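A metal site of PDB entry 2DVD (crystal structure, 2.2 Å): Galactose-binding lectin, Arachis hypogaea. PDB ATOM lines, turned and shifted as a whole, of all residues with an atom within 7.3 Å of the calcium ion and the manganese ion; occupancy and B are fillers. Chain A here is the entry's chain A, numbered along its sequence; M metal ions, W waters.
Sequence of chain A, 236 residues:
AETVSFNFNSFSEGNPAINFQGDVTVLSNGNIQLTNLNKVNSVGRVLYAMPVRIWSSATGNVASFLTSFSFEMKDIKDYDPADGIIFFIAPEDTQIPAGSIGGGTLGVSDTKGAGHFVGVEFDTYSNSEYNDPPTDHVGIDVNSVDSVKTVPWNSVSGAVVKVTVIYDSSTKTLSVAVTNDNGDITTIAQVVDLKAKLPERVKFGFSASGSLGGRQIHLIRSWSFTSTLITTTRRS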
ATOM      1  N   ASP A  83       0.512   1.137   6.527  1.00  0.00           N
ATOM      2  CA  ASP A  83      -0.591   1.742   7.276  1.00  0.00           C
ATOM      3  C   ASP A  83      -0.705   1.266   8.726  1.00  0.00           C
ATOM      4  O   ASP A  83      -1.419   1.880   9.516  1.00  0.00           O
ATOM      5  CB  ASP A  83      -1.915   1.464   6.562  1.00  0.00           C
ATOM      6  CG  ASP A  83      -2.192   2.461   5.458  1.00  0.00           C
ATOM      7  OD1 ASP A  83      -2.828   3.503   5.758  1.00  0.00           O
ATOM      8  OD2 ASP A  83      -1.765   2.232   4.307  1.00  0.00           O
ATOM      9  N   GLY A  84      -0.032   0.175   9.071  1.00  0.00           N
ATOM     10  CA  GLY A  84      -0.108  -0.312  10.439  1.00  0.00           C
ATOM     11  C   GLY A  84      -0.422  -1.792  10.565  1.00  0.00           C
ATOM     12  O   GLY A  84      -0.624  -2.482   9.568  1.00  0.00           O
ATOM     13  N   GLY A 103      -4.280  -0.372   2.465  1.00  0.00           N
ATOM     14  CA  GLY A 103      -4.252   0.926   3.109  1.00  0.00           C
ATOM     15  C   GLY A 103      -4.892   0.987   4.473  1.00  0.00           C
ATOM     16  O   GLY A 103      -4.607   0.165   5.350  1.00  0.00           O
ATOM     17  N   GLY A 104      -5.778   1.969   4.662  1.00  0.00           N
ATOM     18  CA  GLY A 104      -6.452   2.140   5.941  1.00  0.00           C
ATOM     19  C   GLY A 104      -7.349   1.002   6.392  1.00  0.00           C
ATOM     20  O   GLY A 104      -7.754   0.968   7.555  1.00  0.00           O
ATOM     21  N   THR A 105      -7.674   0.083   5.494  1.00  0.00           N
ATOM     22  CA  THR A 105      -8.524  -1.047   5.855  1.00  0.00           C
ATOM     23  C   THR A 105      -7.763  -2.078   6.698  1.00  0.00           C
ATOM     24  O   THR A 105      -8.356  -2.987   7.265  1.00  0.00           O
ATOM     25  CB  THR A 105      -9.041  -1.793   4.606  1.00  0.00           C
ATOM     26  OG1 THR A 105      -7.946  -2.453   3.956  1.00  0.00           O
ATOM     27  CG2 THR A 105      -9.684  -0.815   3.636  1.00  0.00           C
ATOM     28  N   LEU A 106      -6.438  -1.919   6.757  1.00  0.00           N
ATOM     29  CA  LEU A 106      -5.562  -2.812   7.519  1.00  0.00           C
ATOM     30  C   LEU A 106      -5.688  -4.273   7.104  1.00  0.00           C
ATOM     31  O   LEU A 106      -5.235  -5.175   7.817  1.00  0.00           O
ATOM     32  CB  LEU A 106      -5.832  -2.671   9.013  1.00  0.00           C
ATOM     33  CG  LEU A 106      -5.614  -1.257   9.584  1.00  0.00           C
ATOM     34  CD1 LEU A 106      -5.802  -1.277  11.100  1.00  0.00           C
ATOM     35  CD2 LEU A 106      -4.224  -0.775   9.211  1.00  0.00           C
ATOM     36  N   GLU A 121      -5.733  -2.406  16.890  1.00  0.00           N
ATOM     37  CA  GLU A 121      -4.898  -1.853  15.835  1.00  0.00           C
ATOM     38  C   GLU A 121      -3.808  -0.912  16.308  1.00  0.00           C
ATOM     39  O   GLU A 121      -3.946  -0.197  17.312  1.00  0.00           O
ATOM     40  CB  GLU A 121      -5.787  -1.137  14.802  1.00  0.00           C
ATOM     41  CG  GLU A 121      -6.601  -0.010  15.381  1.00  0.00           C
ATOM     42  CD  GLU A 121      -7.147   0.925  14.325  1.00  0.00           C
ATOM     43  OE1 GLU A 121      -7.946   0.471  13.476  1.00  0.00           O
ATOM     44  OE2 GLU A 121      -6.774   2.107  14.341  1.00  0.00           O
ATOM     45  N   PHE A 122      -2.711  -0.930  15.569  1.00  0.00           N
ATOM     46  CA  PHE A 122      -1.539  -0.114  15.805  1.00  0.00           C
ATOM     47  C   PHE A 122      -1.416   0.634  14.485  1.00  0.00           C
ATOM     48  O   PHE A 122      -0.710   0.219  13.572  1.00  0.00           O
ATOM     49  CB  PHE A 122      -0.348  -1.023  16.082  1.00  0.00           C
ATOM     50  CG  PHE A 122      -0.576  -1.927  17.267  1.00  0.00           C
ATOM     51  CD1 PHE A 122      -0.343  -1.469  18.557  1.00  0.00           C
ATOM     52  CD2 PHE A 122      -1.093  -3.206  17.094  1.00  0.00           C
ATOM     53  CE1 PHE A 122      -0.626  -2.277  19.671  1.00  0.00           C
ATOM     54  CE2 PHE A 122      -1.379  -4.027  18.190  1.00  0.00           C
ATOM     55  CZ  PHE A 122      -1.144  -3.556  19.476  1.00  0.00           C
ATOM     56  N   ASP A 123      -2.175   1.715  14.420  1.00  0.00           N
ATOM     57  CA  ASP A 123      -2.326   2.580  13.266  1.00  0.00           C
ATOM     58  C   ASP A 123      -1.278   3.675  13.134  1.00  0.00           C
ATOM     59  O   ASP A 123      -1.087   4.466  14.050  1.00  0.00           O
ATOM     60  CB  ASP A 123      -3.705   3.217  13.346  1.00  0.00           C
ATOM     61  CG  ASP A 123      -4.251   3.573  12.019  1.00  0.00           C
ATOM     62  OD1 ASP A 123      -3.469   4.054  11.168  1.00  0.00           O
ATOM     63  OD2 ASP A 123      -5.466   3.380  11.821  1.00  0.00           O
ATOM     64  N   THR A 124      -0.634   3.748  11.978  1.00  0.00           N
ATOM     65  CA  THR A 124       0.413   4.746  11.763  1.00  0.00           C
ATOM     66  C   THR A 124       0.100   5.791  10.695  1.00  0.00           C
ATOM     67  O   THR A 124       0.984   6.498  10.241  1.00  0.00           O
ATOM     68  CB  THR A 124       1.749   4.069  11.385  1.00  0.00           C
ATOM     69  OG1 THR A 124       1.677   3.587  10.042  1.00  0.00           O
ATOM     70  CG2 THR A 124       2.025   2.890  12.317  1.00  0.00           C
ATOM     71  N   TYR A 125      -1.164   5.867  10.279  1.00  0.00           N
ATOM     72  CA  TYR A 125      -1.551   6.849   9.263  1.00  0.00           C
ATOM     73  C   TYR A 125      -2.982   7.306   9.498  1.00  0.00           C
ATOM     74  O   TYR A 125      -3.861   6.494   9.743  1.00  0.00           O
ATOM     75  CB  TYR A 125      -1.435   6.253   7.859  1.00  0.00           C
ATOM     76  CG  TYR A 125      -1.735   7.270   6.782  1.00  0.00           C
ATOM     77  CD1 TYR A 125      -3.050   7.553   6.418  1.00  0.00           C
ATOM     78  CD2 TYR A 125      -0.712   7.998   6.182  1.00  0.00           C
ATOM     79  CE1 TYR A 125      -3.339   8.553   5.489  1.00  0.00           C
ATOM     80  CE2 TYR A 125      -0.985   8.998   5.257  1.00  0.00           C
ATOM     81  CZ  TYR A 125      -2.301   9.268   4.920  1.00  0.00           C
ATOM     82  OH  TYR A 125      -2.573  10.268   4.017  1.00  0.00           O
ATOM     83  N   SER A 126      -3.218   8.619   9.427  1.00  0.00           N
ATOM     84  CA  SER A 126      -4.561   9.123   9.677  1.00  0.00           C
ATOM     85  C   SER A 126      -5.508   9.112   8.468  1.00  0.00           C
ATOM     86  O   SER A 126      -5.408   9.953   7.573  1.00  0.00           O
ATOM     87  CB  SER A 126      -4.473  10.546  10.246  1.00  0.00           C
ATOM     88  OG  SER A 126      -5.733  10.985  10.706  1.00  0.00           O
ATOM     89  N   ASN A 127      -6.434   8.148   8.461  1.00  0.00           N
ATOM     90  CA  ASN A 127      -7.434   8.029   7.398  1.00  0.00           C
ATOM     91  C   ASN A 127      -8.702   8.728   7.863  1.00  0.00           C
ATOM     92  O   ASN A 127      -9.432   8.210   8.714  1.00  0.00           O
ATOM     93  CB  ASN A 127      -7.775   6.555   7.126  1.00  0.00           C
ATOM     94  CG  ASN A 127      -6.648   5.809   6.454  1.00  0.00           C
ATOM     95  OD1 ASN A 127      -5.660   5.486   7.076  1.00  0.00           O
ATOM     96  ND2 ASN A 127      -6.804   5.548   5.150  1.00  0.00           N
ATOM     97  N   SER A 128      -8.969   9.912   7.311  1.00  0.00           N
ATOM     98  CA  SER A 128     -10.154  10.668   7.689  1.00  0.00           C
ATOM     99  C   SER A 128     -11.431   9.913   7.334  1.00  0.00           C
ATOM    100  O   SER A 128     -12.419   9.994   8.052  1.00  0.00           O
ATOM    101  CB  SER A 128     -10.166  12.036   7.004  1.00  0.00           C
ATOM    102  OG  SER A 128     -10.178  11.909   5.597  1.00  0.00           O
ATOM    103  N   GLU A 129     -11.404   9.160   6.243  1.00  0.00           N
ATOM    104  CA  GLU A 129     -12.585   8.411   5.832  1.00  0.00           C
ATOM    105  C   GLU A 129     -12.991   7.375   6.875  1.00  0.00           C
ATOM    106  O   GLU A 129     -14.083   6.806   6.790  1.00  0.00           O
ATOM    107  CB  GLU A 129     -12.376   7.721   4.472  1.00  0.00           C
ATOM    108  CG  GLU A 129     -11.362   6.596   4.483  1.00  0.00           C
ATOM    109  CD  GLU A 129      -9.941   7.061   4.204  1.00  0.00           C
ATOM    110  OE1 GLU A 129      -9.590   8.191   4.620  1.00  0.00           O
ATOM    111  OE2 GLU A 129      -9.179   6.297   3.585  1.00  0.00           O
ATOM    112  N   TYR A 130     -12.118   7.119   7.857  1.00  0.00           N
ATOM    113  CA  TYR A 130     -12.413   6.158   8.919  1.00  0.00           C
ATOM    114  C   TYR A 130     -12.382   6.830  10.291  1.00  0.00           C
ATOM    115  O   TYR A 130     -12.281   6.161  11.318  1.00  0.00           O
ATOM    116  CB  TYR A 130     -11.418   4.997   8.904  1.00  0.00           C
ATOM    117  CG  TYR A 130     -11.355   4.244   7.593  1.00  0.00           C
ATOM    118  CD1 TYR A 130     -12.521   3.878   6.926  1.00  0.00           C
ATOM    119  CD2 TYR A 130     -10.131   3.901   7.030  1.00  0.00           C
ATOM    120  CE1 TYR A 130     -12.462   3.183   5.713  1.00  0.00           C
ATOM    121  CE2 TYR A 130     -10.056   3.216   5.830  1.00  0.00           C
ATOM    122  CZ  TYR A 130     -11.226   2.848   5.176  1.00  0.00           C
ATOM    123  OH  TYR A 130     -11.146   2.179   3.980  1.00  0.00           O
ATOM    124  N   ASN A 131     -12.453   8.158  10.279  1.00  0.00           N
ATOM    125  CA  ASN A 131     -12.444   8.959  11.498  1.00  0.00           C
ATOM    126  C   ASN A 131     -11.262   8.707  12.433  1.00  0.00           C
ATOM    127  O   ASN A 131     -11.426   8.679  13.658  1.00  0.00           O
ATOM    128  CB  ASN A 131     -13.757   8.771  12.259  1.00  0.00           C
ATOM    129  CG  ASN A 131     -14.947   9.283  11.477  1.00  0.00           C
ATOM    130  OD1 ASN A 131     -14.983  10.442  11.046  1.00  0.00           O
ATOM    131  ND2 ASN A 131     -15.946   8.427  11.300  1.00  0.00           N
ATOM    132  N   ASP A 132     -10.079   8.505  11.869  1.00  0.00           N
ATOM    133  CA  ASP A 132      -8.898   8.289  12.691  1.00  0.00           C
ATOM    134  C   ASP A 132      -8.509   9.553  13.413  1.00  0.00           C
ATOM    135  O   ASP A 132      -8.748  10.659  12.928  1.00  0.00           O
ATOM    136  CB  ASP A 132      -7.683   7.892  11.843  1.00  0.00           C
ATOM    137  CG  ASP A 132      -7.716   6.458  11.411  1.00  0.00           C
ATOM    138  OD1 ASP A 132      -8.068   5.603  12.240  1.00  0.00           O
ATOM    139  OD2 ASP A 132      -7.365   6.189  10.249  1.00  0.00           O
ATOM    140  N   PRO A 133      -7.916   9.409  14.610  1.00  0.00           N
ATOM    141  CA  PRO A 133      -7.514  10.622  15.318  1.00  0.00           C
ATOM    142  C   PRO A 133      -6.357  11.187  14.479  1.00  0.00           C
ATOM    143  O   PRO A 133      -5.837  10.514  13.601  1.00  0.00           O
ATOM    144  CB  PRO A 133      -7.083  10.079  16.694  1.00  0.00           C
ATOM    145  CG  PRO A 133      -6.672   8.667  16.400  1.00  0.00           C
ATOM    146  CD  PRO A 133      -7.723   8.211  15.436  1.00  0.00           C
ATOM    147  N   THR A 135      -3.097  11.713  15.103  1.00  0.00           N
ATOM    148  CA  THR A 135      -1.764  11.104  15.194  1.00  0.00           C
ATOM    149  C   THR A 135      -1.814   9.586  15.351  1.00  0.00           C
ATOM    150  O   THR A 135      -2.882   9.009  15.485  1.00  0.00           O
ATOM    151  CB  THR A 135      -0.959  11.684  16.377  1.00  0.00           C
ATOM    152  OG1 THR A 135      -1.468  11.169  17.616  1.00  0.00           O
ATOM    153  CG2 THR A 135      -1.047  13.206  16.394  1.00  0.00           C
ATOM    154  N   HIS A 137      -1.890   5.888  16.723  1.00  0.00           N
ATOM    155  CA  HIS A 137      -2.736   5.472  17.821  1.00  0.00           C
ATOM    156  C   HIS A 137      -2.976   3.970  17.887  1.00  0.00           C
ATOM    157  O   HIS A 137      -2.800   3.257  16.900  1.00  0.00           O
ATOM    158  CB  HIS A 137      -4.084   6.167  17.689  1.00  0.00           C
ATOM    159  CG  HIS A 137      -4.725   5.952  16.359  1.00  0.00           C
ATOM    160  ND1 HIS A 137      -4.262   6.556  15.204  1.00  0.00           N
ATOM    161  CD2 HIS A 137      -5.747   5.153  15.972  1.00  0.00           C
ATOM    162  CE1 HIS A 137      -4.985   6.140  14.174  1.00  0.00           C
ATOM    163  NE2 HIS A 137      -5.886   5.289  14.622  1.00  0.00           N
ATOM    164  N   VAL A 138      -3.384   3.524  19.061  1.00  0.00           N
ATOM    165  CA  VAL A 138      -3.727   2.133  19.275  1.00  0.00           C
ATOM    166  C   VAL A 138      -5.256   2.210  19.361  1.00  0.00           C
ATOM    167  O   VAL A 138      -5.799   3.122  19.987  1.00  0.00           O
ATOM    168  CB  VAL A 138      -3.150   1.604  20.594  1.00  0.00           C
ATOM    169  CG1 VAL A 138      -3.574   0.147  20.807  1.00  0.00           C
ATOM    170  CG2 VAL A 138      -1.634   1.700  20.564  1.00  0.00           C
ATOM    171  N   GLY A 139      -5.945   1.275  18.731  1.00  0.00           N
ATOM    172  CA  GLY A 139      -7.398   1.318  18.772  1.00  0.00           C
ATOM    173  C   GLY A 139      -8.058  -0.021  18.974  1.00  0.00           C
ATOM    174  O   GLY A 139      -7.497  -1.066  18.663  1.00  0.00           O
ATOM    175  N   ASP A 141     -11.097  -2.171  17.773  1.00  0.00           N
ATOM    176  CA  ASP A 141     -12.059  -2.228  16.685  1.00  0.00           C
ATOM    177  C   ASP A 141     -13.053  -3.371  16.808  1.00  0.00           C
ATOM    178  O   ASP A 141     -12.710  -4.467  17.231  1.00  0.00           O
ATOM    179  CB  ASP A 141     -11.324  -2.370  15.338  1.00  0.00           C
ATOM    180  CG  ASP A 141     -10.299  -1.278  15.104  1.00  0.00           C
ATOM    181  OD1 ASP A 141     -10.331  -0.239  15.806  1.00  0.00           O
ATOM    182  OD2 ASP A 141      -9.460  -1.459  14.198  1.00  0.00           O
ATOM    183  N   VAL A 145     -12.839  -0.420  11.099  1.00  0.00           N
ATOM    184  CA  VAL A 145     -11.569   0.269  11.352  1.00  0.00           C
ATOM    185  C   VAL A 145     -11.856   1.668  11.867  1.00  0.00           C
ATOM    186  O   VAL A 145     -10.940   2.443  12.150  1.00  0.00           O
ATOM    187  CB  VAL A 145     -10.659   0.318  10.097  1.00  0.00           C
ATOM    188  CG1 VAL A 145     -10.077  -1.074   9.835  1.00  0.00           C
ATOM    189  CG2 VAL A 145     -11.445   0.802   8.895  1.00  0.00           C
ATOM    190  N   ASP A 146     -13.136   2.009  11.980  1.00  0.00           N
ATOM    191  CA  ASP A 146     -13.520   3.282  12.553  1.00  0.00           C
ATOM    192  C   ASP A 146     -13.605   2.837  14.014  1.00  0.00           C
ATOM    193  O   ASP A 146     -14.652   2.418  14.499  1.00  0.00           O
ATOM    194  CB  ASP A 146     -14.890   3.745  12.057  1.00  0.00           C
ATOM    195  CG  ASP A 146     -15.266   5.131  12.570  1.00  0.00           C
ATOM    196  OD1 ASP A 146     -14.943   5.433  13.731  1.00  0.00           O
ATOM    197  OD2 ASP A 146     -15.870   5.919  11.821  1.00  0.00           O
ATOM    198  N   SER A 147     -12.460   2.898  14.691  1.00  0.00           N
ATOM    199  CA  SER A 147     -12.352   2.451  16.068  1.00  0.00           C
ATOM    200  C   SER A 147     -13.443   2.871  17.048  1.00  0.00           C
ATOM    201  O   SER A 147     -13.909   4.017  17.060  1.00  0.00           O
ATOM    202  CB  SER A 147     -10.998   2.870  16.637  1.00  0.00           C
ATOM    203  OG  SER A 147      -9.942   2.281  15.893  1.00  0.00           O
ATOM    204  N   THR A 150      -9.854   4.883  20.745  1.00  0.00           N
ATOM    205  CA  THR A 150      -8.439   4.995  20.426  1.00  0.00           C
ATOM    206  C   THR A 150      -7.704   5.732  21.536  1.00  0.00           C
ATOM    207  O   THR A 150      -8.313   6.369  22.386  1.00  0.00           O
ATOM    208  CB  THR A 150      -8.180   5.774  19.117  1.00  0.00           C
ATOM    209  OG1 THR A 150      -8.429   7.175  19.331  1.00  0.00           O
ATOM    210  CG2 THR A 150      -9.069   5.271  17.993  1.00  0.00           C
HETATM  211 CA    CA M   1      -5.435   4.561   9.495  1.00  0.00          CA
HETATM  212 MN    MN M   2      -7.208   3.915  13.099  1.00  0.00          MN
HETATM  213  O   HOH W   1      -3.536   3.082   8.575  1.00  0.00           O
HETATM  214  O   HOH W   2      -7.150   2.944   9.488  1.00  0.00           O
HETATM  215  O   HOH W   3      -8.420   2.276  11.766  1.00  0.00           O
HETATM  216  O   HOH W   4      -8.952   4.292  14.528  1.00  0.00           O
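The nearest printed residue that does not touch the calcium ion is Gly 104 (4.4 Å).
Water W3 bridges OE1 of Glu 121 (2.5 Å) and O of Val 145 (2.6 Å).
The calcium ion is bound by water W2, the backbone carbonyl oxygen (O) of Tyr 125, water W1, the side-chain amide oxygen (OD1) of Asn 127, the side-chain carboxylate (OD2) of Asp 123, the side-chain carboxylate (OD1) of Asp 123 and the side-chain carboxylate (OD2) of Asp 132.
The calcium ion has seven donor atoms within binding distance.
The manganese ion is bound by the side-chain carboxylate (OD1) of Asp 132, the side-chain carboxylate (OD2) of Asp 123, the side-chain carboxylate (OE2) of Glu 121, water W4, water W3 and a ring nitrogen (NE2) of His 137.
The side-chain carboxylate (OD2) of Asp 141 lies close to the side-chain carboxylate (OE1) of Glu 121, at 2.6 Å.
The backbone carbonyl oxygen of Gly 139 is in hydrogen-bond range of the backbone NH of Glu 121 (2.8 Å).
A ring nitrogen (ND1) of His 137 sits at hydrogen-bond distance from the backbone carbonyl oxygen (O) of Thr 135 (2.8 Å).
The side-chain amide nitrogen (ND2) of Asn 127 sits at hydrogen-bond distance from the side-chain carboxylate (OE2) of Glu 129 (2.9 Å).
Within 4 Å of the manganese ion: Glu 121, Asp 123, Asp 132 and His 137.
Along chain A the residues within 4 Å of the manganese ion span positions 121 to 137.
The nearest printed residue that does not touch the manganese ion is Val 145 (4.1 Å).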
